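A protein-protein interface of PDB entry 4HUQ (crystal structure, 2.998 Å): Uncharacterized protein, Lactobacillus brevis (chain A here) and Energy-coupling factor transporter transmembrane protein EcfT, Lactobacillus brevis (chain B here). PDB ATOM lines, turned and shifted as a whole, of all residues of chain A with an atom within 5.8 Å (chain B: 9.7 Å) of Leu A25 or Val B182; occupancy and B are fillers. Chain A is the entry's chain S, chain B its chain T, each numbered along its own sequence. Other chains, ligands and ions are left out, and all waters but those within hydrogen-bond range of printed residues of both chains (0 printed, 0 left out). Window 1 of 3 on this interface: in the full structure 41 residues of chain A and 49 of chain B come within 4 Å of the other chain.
The side-chain hydroxyl (OG) of Ser A28 sits at hydrogen-bond distance from the backbone carbonyl oxygen (O) of Leu A25, at 2.5 Å.
O of Phe B181 sits at hydrogen-bond distance from OG1 of Thr B184 (3.4 Å).
Among the printed residues, pairs that only touch across the chains: Ala A22 with Ala B178 (3.1 Å), Ala A22 with Val B182 (3.6 Å), Ile A68 with Leu B175 (3.6 Å), Leu A23 with Leu B222 (3.6 Å), Ala A22 with Phe B181 (3.7 Å), Arg A29 with Met B186 (3.7 Å), Leu A23 with Leu B185 (3.7 Å), Met A21 with Ala B178 (3.7 Å), Met A72 with Pro B147 (3.8 Å), Leu A25 with Val B182 (3.8 Å) and Met A21 with Leu B175 (3.99 Å).
Leu A25 touches just one residue of chain B: Val B182.
Of chain A, only Ala A22 (3.6 Å) and Leu A25 (3.8 Å) come within 4 Å of Val B182.
Val A26 touches none of the printed residues of chain B.
Gly A69 touches none of the printed residues of chain B.
Printed residues of chain A within 4 Å of Leu B222: Leu A23.
Printed residues of chain A within 4 Å of Ala B178: Met A21 (3.7 Å) and Ala A22 (3.1 Å).
Ser B176 touches none of the printed residues of chain A.
The nearest residue of chain B that does not touch Leu A25 is Leu B179 (4.2 Å).
The nearest residue of chain A that does not touch Val B182 is Val A26 (4.2 Å).
The nearest printed residue of chain A that does not touch Met B186 is Val A26 (4.1 Å).
Of the 25 printed residues of chain B, 8 touch a printed residue of chain A.
Hydrophobic or aromatic side chains of chain B within 4 Å of the printed part of chain A: Pro B147, Leu B175, Ala B178, Phe B181, Val B182, Leu B185, Met B186 and Leu B222.
Of the 14 printed residues of chain A, 7 touch a printed residue of chain B.
Hydrophobic or aromatic side chains of chain A within 4 Å of the printed part of chain B: Met A21, Ala A22, Leu A23, Leu A25, Ile A68 and Met A72.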
ATOM      1  N   LEU A  20      12.096 -24.825  14.457  1.00  0.00           N
ATOM      2  CA  LEU A  20      13.340 -24.084  14.611  1.00  0.00           C
ATOM      3  C   LEU A  20      13.070 -22.588  14.595  1.00  0.00           C
ATOM      4  O   LEU A  20      13.681 -21.827  15.341  1.00  0.00           O
ATOM      5  CB  LEU A  20      14.329 -24.458  13.510  1.00  0.00           C
ATOM      6  CG  LEU A  20      14.942 -25.853  13.616  1.00  0.00           C
ATOM      7  CD1 LEU A  20      14.599 -26.681  12.389  1.00  0.00           C
ATOM      8  CD2 LEU A  20      16.447 -25.764  13.801  1.00  0.00           C
ATOM      9  N   MET A  21      12.155 -22.169  13.731  1.00  0.00           N
ATOM     10  CA  MET A  21      11.769 -20.771  13.645  1.00  0.00           C
ATOM     11  C   MET A  21      11.156 -20.328  14.964  1.00  0.00           C
ATOM     12  O   MET A  21      11.433 -19.234  15.448  1.00  0.00           O
ATOM     13  CB  MET A  21      10.767 -20.563  12.510  1.00  0.00           C
ATOM     14  CG  MET A  21      11.363 -20.682  11.117  1.00  0.00           C
ATOM     15  SD  MET A  21      10.104 -20.635   9.831  1.00  0.00           S
ATOM     16  CE  MET A  21       9.173 -19.188  10.322  1.00  0.00           C
ATOM     17  N   ALA A  22      10.329 -21.187  15.551  1.00  0.00           N
ATOM     18  CA  ALA A  22       9.772 -20.916  16.871  1.00  0.00           C
ATOM     19  C   ALA A  22      10.896 -20.848  17.899  1.00  0.00           C
ATOM     20  O   ALA A  22      10.890 -20.005  18.792  1.00  0.00           O
ATOM     21  CB  ALA A  22       8.764 -21.984  17.252  1.00  0.00           C
ATOM     22  N   LEU A  23      11.858 -21.751  17.757  1.00  0.00           N
ATOM     23  CA  LEU A  23      13.029 -21.796  18.612  1.00  0.00           C
ATOM     24  C   LEU A  23      13.868 -20.526  18.490  1.00  0.00           C
ATOM     25  O   LEU A  23      14.429 -20.049  19.481  1.00  0.00           O
ATOM     26  CB  LEU A  23      13.860 -23.024  18.242  1.00  0.00           C
ATOM     27  CG  LEU A  23      14.853 -23.592  19.247  1.00  0.00           C
ATOM     28  CD1 LEU A  23      14.289 -23.481  20.637  1.00  0.00           C
ATOM     29  CD2 LEU A  23      15.108 -25.042  18.899  1.00  0.00           C
ATOM     30  N   GLN A  24      13.939 -19.983  17.273  1.00  0.00           N
ATOM     31  CA  GLN A  24      14.743 -18.793  16.998  1.00  0.00           C
ATOM     32  C   GLN A  24      14.168 -17.562  17.684  1.00  0.00           C
ATOM     33  O   GLN A  24      14.908 -16.767  18.261  1.00  0.00           O
ATOM     34  CB  GLN A  24      14.870 -18.532  15.495  1.00  0.00           C
ATOM     35  CG  GLN A  24      16.174 -17.832  15.135  1.00  0.00           C
ATOM     36  CD  GLN A  24      16.150 -17.119  13.786  1.00  0.00           C
ATOM     37  OE1 GLN A  24      16.263 -15.893  13.725  1.00  0.00           O
ATOM     38  NE2 GLN A  24      16.032 -17.884  12.699  1.00  0.00           N
ATOM     39  N   LEU A  25      12.848 -17.415  17.617  1.00  0.00           N
ATOM     40  CA  LEU A  25      12.155 -16.343  18.314  1.00  0.00           C
ATOM     41  C   LEU A  25      12.396 -16.356  19.833  1.00  0.00           C
ATOM     42  O   LEU A  25      12.499 -15.301  20.453  1.00  0.00           O
ATOM     43  CB  LEU A  25      10.662 -16.412  18.016  1.00  0.00           C
ATOM     44  CG  LEU A  25      10.331 -16.243  16.533  1.00  0.00           C
ATOM     45  CD1 LEU A  25       8.944 -16.826  16.156  1.00  0.00           C
ATOM     46  CD2 LEU A  25      10.449 -14.772  16.138  1.00  0.00           C
ATOM     47  N   VAL A  26      12.491 -17.539  20.433  1.00  0.00           N
ATOM     48  CA  VAL A  26      12.666 -17.638  21.884  1.00  0.00           C
ATOM     49  C   VAL A  26      14.023 -17.095  22.303  1.00  0.00           C
ATOM     50  O   VAL A  26      14.122 -16.153  23.085  1.00  0.00           O
ATOM     51  CB  VAL A  26      12.524 -19.089  22.373  1.00  0.00           C
ATOM     52  CG1 VAL A  26      12.790 -19.168  23.857  1.00  0.00           C
ATOM     53  CG2 VAL A  26      11.136 -19.617  22.061  1.00  0.00           C
ATOM     54  N   ILE A  27      15.067 -17.694  21.756  1.00  0.00           N
ATOM     55  CA  ILE A  27      16.438 -17.245  21.964  1.00  0.00           C
ATOM     56  C   ILE A  27      16.652 -15.756  21.648  1.00  0.00           C
ATOM     57  O   ILE A  27      17.600 -15.139  22.126  1.00  0.00           O
ATOM     58  CB  ILE A  27      17.368 -18.125  21.112  1.00  0.00           C
ATOM     59  CG1 ILE A  27      17.124 -19.590  21.483  1.00  0.00           C
ATOM     60  CG2 ILE A  27      18.832 -17.724  21.251  1.00  0.00           C
ATOM     61  CD1 ILE A  27      18.108 -20.546  20.908  1.00  0.00           C
ATOM     62  N   SER A  28      15.762 -15.182  20.846  1.00  0.00           N
ATOM     63  CA  SER A  28      15.886 -13.786  20.449  1.00  0.00           C
ATOM     64  C   SER A  28      15.379 -12.897  21.555  1.00  0.00           C
ATOM     65  O   SER A  28      15.687 -11.706  21.592  1.00  0.00           O
ATOM     66  CB  SER A  28      15.103 -13.494  19.162  1.00  0.00           C
ATOM     67  OG  SER A  28      13.706 -13.365  19.393  1.00  0.00           O
ATOM     68  N   ARG A  29      14.590 -13.482  22.453  1.00  0.00           N
ATOM     69  CA  ARG A  29      14.074 -12.746  23.595  1.00  0.00           C
ATOM     70  C   ARG A  29      15.167 -12.641  24.651  1.00  0.00           C
ATOM     71  O   ARG A  29      14.993 -11.990  25.682  1.00  0.00           O
ATOM     72  CB  ARG A  29      12.851 -13.449  24.187  1.00  0.00           C
ATOM     73  CG  ARG A  29      11.720 -13.722  23.213  1.00  0.00           C
ATOM     74  CD  ARG A  29      10.371 -13.590  23.907  1.00  0.00           C
ATOM     75  NE  ARG A  29      10.133 -12.210  24.320  1.00  0.00           N
ATOM     76  CZ  ARG A  29       9.588 -11.852  25.478  1.00  0.00           C
ATOM     77  NH1 ARG A  29       9.208 -12.779  26.351  1.00  0.00           N
ATOM     78  NH2 ARG A  29       9.417 -10.563  25.758  1.00  0.00           N
ATOM     79  N   VAL A  65      11.489 -14.994   9.581  1.00  0.00           N
ATOM     80  CA  VAL A  65      11.789 -14.822  10.999  1.00  0.00           C
ATOM     81  C   VAL A  65      12.253 -13.405  11.331  1.00  0.00           C
ATOM     82  O   VAL A  65      11.843 -12.833  12.343  1.00  0.00           O
ATOM     83  CB  VAL A  65      12.836 -15.840  11.505  1.00  0.00           C
ATOM     84  CG1 VAL A  65      13.092 -15.637  12.975  1.00  0.00           C
ATOM     85  CG2 VAL A  65      12.350 -17.248  11.288  1.00  0.00           C
ATOM     86  N   ILE A  68       8.797 -11.308  10.902  1.00  0.00           N
ATOM     87  CA  ILE A  68       7.786 -11.606  11.901  1.00  0.00           C
ATOM     88  C   ILE A  68       8.345 -11.213  13.258  1.00  0.00           C
ATOM     89  O   ILE A  68       7.600 -10.884  14.176  1.00  0.00           O
ATOM     90  CB  ILE A  68       7.347 -13.108  11.896  1.00  0.00           C
ATOM     91  CG1 ILE A  68       5.975 -13.266  12.554  1.00  0.00           C
ATOM     92  CG2 ILE A  68       8.384 -14.014  12.584  1.00  0.00           C
ATOM     93  CD1 ILE A  68       4.917 -12.401  11.927  1.00  0.00           C
ATOM     94  N   GLY A  69       9.669 -11.213  13.362  1.00  0.00           N
ATOM     95  CA  GLY A  69      10.330 -11.056  14.641  1.00  0.00           C
ATOM     96  C   GLY A  69      10.408  -9.607  15.043  1.00  0.00           C
ATOM     97  O   GLY A  69       9.910  -9.222  16.097  1.00  0.00           O
ATOM     98  N   MET A  72       7.121  -8.200  15.895  1.00  0.00           N
ATOM     99  CA  MET A  72       6.461  -8.641  17.121  1.00  0.00           C
ATOM    100  C   MET A  72       7.085  -8.084  18.376  1.00  0.00           C
ATOM    101  O   MET A  72       6.429  -8.005  19.407  1.00  0.00           O
ATOM    102  CB  MET A  72       6.419 -10.160  17.205  1.00  0.00           C
ATOM    103  CG  MET A  72       5.230 -10.754  16.501  1.00  0.00           C
ATOM    104  SD  MET A  72       5.454 -12.507  16.326  1.00  0.00           S
ATOM    105  CE  MET A  72       5.615 -12.965  18.043  1.00  0.00           C
ATOM    106  N   PHE B  20       4.251 -14.577  23.842  1.00  0.00           N
ATOM    107  CA  PHE B  20       4.776 -14.018  22.603  1.00  0.00           C
ATOM    108  C   PHE B  20       5.383 -12.638  22.838  1.00  0.00           C
ATOM    109  O   PHE B  20       6.105 -12.114  21.990  1.00  0.00           O
ATOM    110  CB  PHE B  20       3.676 -13.942  21.543  1.00  0.00           C
ATOM    111  CG  PHE B  20       2.334 -13.554  22.092  1.00  0.00           C
ATOM    112  CD1 PHE B  20       1.301 -14.473  22.143  1.00  0.00           C
ATOM    113  CD2 PHE B  20       2.105 -12.270  22.555  1.00  0.00           C
ATOM    114  CE1 PHE B  20       0.064 -14.118  22.644  1.00  0.00           C
ATOM    115  CE2 PHE B  20       0.871 -11.909  23.058  1.00  0.00           C
ATOM    116  CZ  PHE B  20      -0.152 -12.835  23.104  1.00  0.00           C
ATOM    117  N   GLY B  21       5.085 -12.056  23.994  1.00  0.00           N
ATOM    118  CA  GLY B  21       5.613 -10.753  24.346  1.00  0.00           C
ATOM    119  C   GLY B  21       4.541  -9.803  24.839  1.00  0.00           C
ATOM    120  O   GLY B  21       4.482  -8.650  24.415  1.00  0.00           O
ATOM    121  N   ARG B  22       3.692 -10.286  25.739  1.00  0.00           N
ATOM    122  CA  ARG B  22       2.626  -9.464  26.298  1.00  0.00           C
ATOM    123  C   ARG B  22       2.621  -8.090  25.645  1.00  0.00           C
ATOM    124  O   ARG B  22       3.173  -7.133  26.188  1.00  0.00           O
ATOM    125  CB  ARG B  22       2.794  -9.322  27.813  1.00  0.00           C
ATOM    126  CG  ARG B  22       2.843 -10.642  28.566  1.00  0.00           C
ATOM    127  CD  ARG B  22       3.946 -10.640  29.611  1.00  0.00           C
ATOM    128  NE  ARG B  22       4.240 -11.985  30.098  1.00  0.00           N
ATOM    129  CZ  ARG B  22       4.851 -12.247  31.250  1.00  0.00           C
ATOM    130  NH1 ARG B  22       5.237 -11.254  32.039  1.00  0.00           N
ATOM    131  NH2 ARG B  22       5.077 -13.502  31.612  1.00  0.00           N
ATOM    132  N   PRO B 147      -0.161 -10.928  16.971  1.00  0.00           N
ATOM    133  CA  PRO B 147       0.828 -11.554  16.082  1.00  0.00           C
ATOM    134  C   PRO B 147       0.158 -12.551  15.148  1.00  0.00           C
ATOM    135  O   PRO B 147       0.486 -12.622  13.964  1.00  0.00           O
ATOM    136  CB  PRO B 147       1.766 -12.300  17.043  1.00  0.00           C
ATOM    137  CG  PRO B 147       1.478 -11.767  18.381  1.00  0.00           C
ATOM    138  CD  PRO B 147       0.052 -11.300  18.375  1.00  0.00           C
ATOM    139  N   ALA B 151       0.367 -12.354  11.373  1.00  0.00           N
ATOM    140  CA  ALA B 151       0.728 -13.479  10.529  1.00  0.00           C
ATOM    141  C   ALA B 151      -0.328 -13.707   9.446  1.00  0.00           C
ATOM    142  O   ALA B 151       0.012 -13.897   8.274  1.00  0.00           O
ATOM    143  CB  ALA B 151       0.933 -14.732  11.371  1.00  0.00           C
ATOM    144  N   MET B 174       4.656 -22.918   7.787  1.00  0.00           N
ATOM    145  CA  MET B 174       5.851 -22.896   8.625  1.00  0.00           C
ATOM    146  C   MET B 174       5.760 -21.883   9.760  1.00  0.00           C
ATOM    147  O   MET B 174       6.036 -22.196  10.919  1.00  0.00           O
ATOM    148  CB  MET B 174       7.072 -22.565   7.782  1.00  0.00           C
ATOM    149  CG  MET B 174       7.261 -23.516   6.655  1.00  0.00           C
ATOM    150  SD  MET B 174       8.970 -23.625   6.145  1.00  0.00           S
ATOM    151  CE  MET B 174       8.812 -24.912   4.912  1.00  0.00           C
ATOM    152  N   LEU B 175       5.378 -20.663   9.408  1.00  0.00           N
ATOM    153  CA  LEU B 175       5.209 -19.603  10.384  1.00  0.00           C
ATOM    154  C   LEU B 175       4.109 -19.952  11.384  1.00  0.00           C
ATOM    155  O   LEU B 175       4.282 -19.762  12.587  1.00  0.00           O
ATOM    156  CB  LEU B 175       4.876 -18.297   9.665  1.00  0.00           C
ATOM    157  CG  LEU B 175       4.644 -17.022  10.475  1.00  0.00           C
ATOM    158  CD1 LEU B 175       5.922 -16.580  11.155  1.00  0.00           C
ATOM    159  CD2 LEU B 175       4.121 -15.943   9.545  1.00  0.00           C
ATOM    160  N   SER B 176       2.983 -20.458  10.882  1.00  0.00           N
ATOM    161  CA  SER B 176       1.864 -20.851  11.734  1.00  0.00           C
ATOM    162  C   SER B 176       2.301 -21.870  12.786  1.00  0.00           C
ATOM    163  O   SER B 176       2.014 -21.714  13.980  1.00  0.00           O
ATOM    164  CB  SER B 176       0.729 -21.424  10.893  1.00  0.00           C
ATOM    165  OG  SER B 176      -0.405 -20.583  10.967  1.00  0.00           O
ATOM    166  N   ILE B 177       2.988 -22.912  12.325  1.00  0.00           N
ATOM    167  CA  ILE B 177       3.632 -23.851  13.219  1.00  0.00           C
ATOM    168  C   ILE B 177       4.548 -23.086  14.170  1.00  0.00           C
ATOM    169  O   ILE B 177       4.436 -23.218  15.388  1.00  0.00           O
ATOM    170  CB  ILE B 177       4.430 -24.920  12.441  1.00  0.00           C
ATOM    171  CG1 ILE B 177       3.559 -26.153  12.184  1.00  0.00           C
ATOM    172  CG2 ILE B 177       5.688 -25.347  13.206  1.00  0.00           C
ATOM    173  CD1 ILE B 177       2.803 -26.118  10.889  1.00  0.00           C
ATOM    174  N   ALA B 178       5.430 -22.267  13.611  1.00  0.00           N
ATOM    175  CA  ALA B 178       6.354 -21.484  14.415  1.00  0.00           C
ATOM    176  C   ALA B 178       5.634 -20.699  15.514  1.00  0.00           C
ATOM    177  O   ALA B 178       6.113 -20.606  16.638  1.00  0.00           O
ATOM    178  CB  ALA B 178       7.165 -20.552  13.534  1.00  0.00           C
ATOM    179  N   LEU B 179       4.469 -20.151  15.209  1.00  0.00           N
ATOM    180  CA  LEU B 179       3.808 -19.307  16.191  1.00  0.00           C
ATOM    181  C   LEU B 179       3.060 -20.070  17.263  1.00  0.00           C
ATOM    182  O   LEU B 179       2.823 -19.524  18.339  1.00  0.00           O
ATOM    183  CB  LEU B 179       2.878 -18.297  15.524  1.00  0.00           C
ATOM    184  CG  LEU B 179       3.632 -17.093  14.972  1.00  0.00           C
ATOM    185  CD1 LEU B 179       2.655 -15.995  14.644  1.00  0.00           C
ATOM    186  CD2 LEU B 179       4.708 -16.624  15.977  1.00  0.00           C
ATOM    187  N   ARG B 180       2.672 -21.313  16.981  1.00  0.00           N
ATOM    188  CA  ARG B 180       1.958 -22.077  17.998  1.00  0.00           C
ATOM    189  C   ARG B 180       2.923 -22.816  18.947  1.00  0.00           C
ATOM    190  O   ARG B 180       2.577 -23.128  20.096  1.00  0.00           O
ATOM    191  CB  ARG B 180       0.917 -23.009  17.382  1.00  0.00           C
ATOM    192  CG  ARG B 180       1.502 -24.200  16.697  1.00  0.00           C
ATOM    193  CD  ARG B 180       0.849 -25.479  17.191  1.00  0.00           C
ATOM    194  NE  ARG B 180       1.156 -25.768  18.589  1.00  0.00           N
ATOM    195  CZ  ARG B 180       1.318 -26.995  19.068  1.00  0.00           C
ATOM    196  NH1 ARG B 180       1.214 -28.039  18.258  1.00  0.00           N
ATOM    197  NH2 ARG B 180       1.589 -27.175  20.348  1.00  0.00           N
ATOM    198  N   PHE B 181       4.143 -23.053  18.474  1.00  0.00           N
ATOM    199  CA  PHE B 181       5.189 -23.627  19.315  1.00  0.00           C
ATOM    200  C   PHE B 181       5.895 -22.646  20.256  1.00  0.00           C
ATOM    201  O   PHE B 181       6.407 -23.049  21.302  1.00  0.00           O
ATOM    202  CB  PHE B 181       6.220 -24.337  18.458  1.00  0.00           C
ATOM    203  CG  PHE B 181       5.857 -25.739  18.161  1.00  0.00           C
ATOM    204  CD1 PHE B 181       5.054 -26.442  19.036  1.00  0.00           C
ATOM    205  CD2 PHE B 181       6.289 -26.353  17.001  1.00  0.00           C
ATOM    206  CE1 PHE B 181       4.701 -27.728  18.770  1.00  0.00           C
ATOM    207  CE2 PHE B 181       5.939 -27.644  16.728  1.00  0.00           C
ATOM    208  CZ  PHE B 181       5.143 -28.335  17.611  1.00  0.00           C
ATOM    209  N   VAL B 182       5.941 -21.374  19.882  1.00  0.00           N
ATOM    210  CA  VAL B 182       6.621 -20.387  20.711  1.00  0.00           C
ATOM    211  C   VAL B 182       6.232 -20.444  22.192  1.00  0.00           C
ATOM    212  O   VAL B 182       7.114 -20.559  23.041  1.00  0.00           O
ATOM    213  CB  VAL B 182       6.508 -18.955  20.153  1.00  0.00           C
ATOM    214  CG1 VAL B 182       6.617 -17.951  21.271  1.00  0.00           C
ATOM    215  CG2 VAL B 182       7.596 -18.717  19.140  1.00  0.00           C
ATOM    216  N   PRO B 183       4.924 -20.390  22.507  1.00  0.00           N
ATOM    217  CA  PRO B 183       4.567 -20.524  23.924  1.00  0.00           C
ATOM    218  C   PRO B 183       4.918 -21.895  24.546  1.00  0.00           C
ATOM    219  O   PRO B 183       5.381 -21.935  25.693  1.00  0.00           O
ATOM    220  CB  PRO B 183       3.057 -20.279  23.928  1.00  0.00           C
ATOM    221  CG  PRO B 183       2.625 -20.604  22.547  1.00  0.00           C
ATOM    222  CD  PRO B 183       3.736 -20.142  21.673  1.00  0.00           C
ATOM    223  N   THR B 184       4.724 -22.997  23.827  1.00  0.00           N
ATOM    224  CA  THR B 184       5.071 -24.280  24.427  1.00  0.00           C
ATOM    225  C   THR B 184       6.572 -24.407  24.669  1.00  0.00           C
ATOM    226  O   THR B 184       6.966 -24.855  25.726  1.00  0.00           O
ATOM    227  CB  THR B 184       4.563 -25.525  23.644  1.00  0.00           C
ATOM    228  OG1 THR B 184       5.593 -25.993  22.770  1.00  0.00           O
ATOM    229  CG2 THR B 184       3.281 -25.236  22.877  1.00  0.00           C
ATOM    230  N   LEU B 185       7.405 -24.010  23.706  1.00  0.00           N
ATOM    231  CA  LEU B 185       8.864 -24.041  23.891  1.00  0.00           C
ATOM    232  C   LEU B 185       9.286 -23.183  25.054  1.00  0.00           C
ATOM    233  O   LEU B 185      10.266 -23.498  25.727  1.00  0.00           O
ATOM    234  CB  LEU B 185       9.605 -23.558  22.648  1.00  0.00           C
ATOM    235  CG  LEU B 185       9.555 -24.490  21.449  1.00  0.00           C
ATOM    236  CD1 LEU B 185      10.561 -24.046  20.413  1.00  0.00           C
ATOM    237  CD2 LEU B 185       9.827 -25.916  21.918  1.00  0.00           C
ATOM    238  N   MET B 186       8.545 -22.094  25.275  1.00  0.00           N
ATOM    239  CA  MET B 186       8.758 -21.194  26.407  1.00  0.00           C
ATOM    240  C   MET B 186       8.419 -21.872  27.727  1.00  0.00           C
ATOM    241  O   MET B 186       9.229 -21.858  28.649  1.00  0.00           O
ATOM    242  CB  MET B 186       7.918 -19.925  26.257  1.00  0.00           C
ATOM    243  CG  MET B 186       8.675 -18.690  25.740  1.00  0.00           C
ATOM    244  SD  MET B 186      10.072 -18.187  26.777  1.00  0.00           S
ATOM    245  CE  MET B 186      10.268 -16.490  26.232  1.00  0.00           C
ATOM    246  N   ASP B 187       7.223 -22.449  27.814  1.00  0.00           N
ATOM    247  CA  ASP B 187       6.816 -23.218  28.993  1.00  0.00           C
ATOM    248  C   ASP B 187       7.820 -24.323  29.288  1.00  0.00           C
ATOM    249  O   ASP B 187       8.138 -24.598  30.455  1.00  0.00           O
ATOM    250  CB  ASP B 187       5.404 -23.807  28.829  1.00  0.00           C
ATOM    251  CG  ASP B 187       4.295 -22.742  28.943  1.00  0.00           C
ATOM    252  OD1 ASP B 187       4.474 -21.756  29.699  1.00  0.00           O
ATOM    253  OD2 ASP B 187       3.239 -22.893  28.280  1.00  0.00           O
ATOM    254  N   GLU B 188       8.341 -24.922  28.222  1.00  0.00           N
ATOM    255  CA  GLU B 188       9.272 -26.045  28.320  1.00  0.00           C
ATOM    256  C   GLU B 188      10.635 -25.564  28.789  1.00  0.00           C
ATOM    257  O   GLU B 188      11.284 -26.191  29.631  1.00  0.00           O
ATOM    258  CB  GLU B 188       9.398 -26.748  26.963  1.00  0.00           C
ATOM    259  CG  GLU B 188      10.289 -27.979  26.950  1.00  0.00           C
ATOM    260  CD  GLU B 188       9.556 -29.232  27.393  1.00  0.00           C
ATOM    261  OE1 GLU B 188       8.449 -29.101  27.967  1.00  0.00           O
ATOM    262  OE2 GLU B 188      10.083 -30.346  27.158  1.00  0.00           O
ATOM    263  N   ALA B 189      11.060 -24.438  28.234  1.00  0.00           N
ATOM    264  CA  ALA B 189      12.342 -23.868  28.592  1.00  0.00           C
ATOM    265  C   ALA B 189      12.411 -23.594  30.100  1.00  0.00           C
ATOM    266  O   ALA B 189      13.431 -23.848  30.736  1.00  0.00           O
ATOM    267  CB  ALA B 189      12.585 -22.610  27.791  1.00  0.00           C
ATOM    268  N   THR B 190      11.316 -23.110  30.675  1.00  0.00           N
ATOM    269  CA  THR B 190      11.290 -22.822  32.106  1.00  0.00           C
ATOM    270  C   THR B 190      11.349 -24.112  32.922  1.00  0.00           C
ATOM    271  O   THR B 190      12.040 -24.153  33.942  1.00  0.00           O
ATOM    272  CB  THR B 190      10.046 -21.978  32.542  1.00  0.00           C
ATOM    273  OG1 THR B 190       8.868 -22.794  32.505  1.00  0.00           O
ATOM    274  CG2 THR B 190       9.833 -20.800  31.618  1.00  0.00           C
ATOM    275  N   LEU B 222      16.307 -28.776  25.281  1.00  0.00           N
ATOM    276  CA  LEU B 222      15.293 -28.025  24.534  1.00  0.00           C
ATOM    277  C   LEU B 222      15.209 -28.407  23.051  1.00  0.00           C
ATOM    278  O   LEU B 222      14.120 -28.644  22.535  1.00  0.00           O
ATOM    279  CB  LEU B 222      15.551 -26.527  24.648  1.00  0.00           C
ATOM    280  CG  LEU B 222      14.330 -25.640  24.901  1.00  0.00           C
ATOM    281  CD1 LEU B 222      14.471 -24.341  24.142  1.00  0.00           C
ATOM    282  CD2 LEU B 222      13.026 -26.349  24.557  1.00  0.00           C
ATOM    283  N   ALA B 226      12.126 -30.155  21.052  1.00  0.00           N
ATOM    284  CA  ALA B 226      11.574 -29.502  19.896  1.00  0.00           C
ATOM    285  C   ALA B 226      11.543 -30.492  18.745  1.00  0.00           C
ATOM    286  O   ALA B 226      10.480 -30.773  18.189  1.00  0.00           O
ATOM    287  CB  ALA B 226      12.401 -28.297  19.548  1.00  0.00           C
ATOM    288  N   ARG B 229       8.964 -33.067  19.370  1.00  0.00           N
ATOM    289  CA  ARG B 229       7.660 -32.452  19.129  1.00  0.00           C
ATOM    290  C   ARG B 229       7.381 -32.294  17.646  1.00  0.00           C
ATOM    291  O   ARG B 229       6.265 -32.539  17.195  1.00  0.00           O
ATOM    292  CB  ARG B 229       7.534 -31.109  19.857  1.00  0.00           C
ATOM    293  CG  ARG B 229       7.343 -31.281  21.342  1.00  0.00           C
ATOM    294  CD  ARG B 229       7.509 -30.000  22.142  1.00  0.00           C
ATOM    295  NE  ARG B 229       7.765 -30.358  23.526  1.00  0.00           N
ATOM    296  CZ  ARG B 229       6.830 -30.743  24.389  1.00  0.00           C
ATOM    297  NH1 ARG B 229       5.559 -30.783  24.019  1.00  0.00           N
ATOM    298  NH2 ARG B 229       7.173 -31.081  25.629  1.00  0.00           N
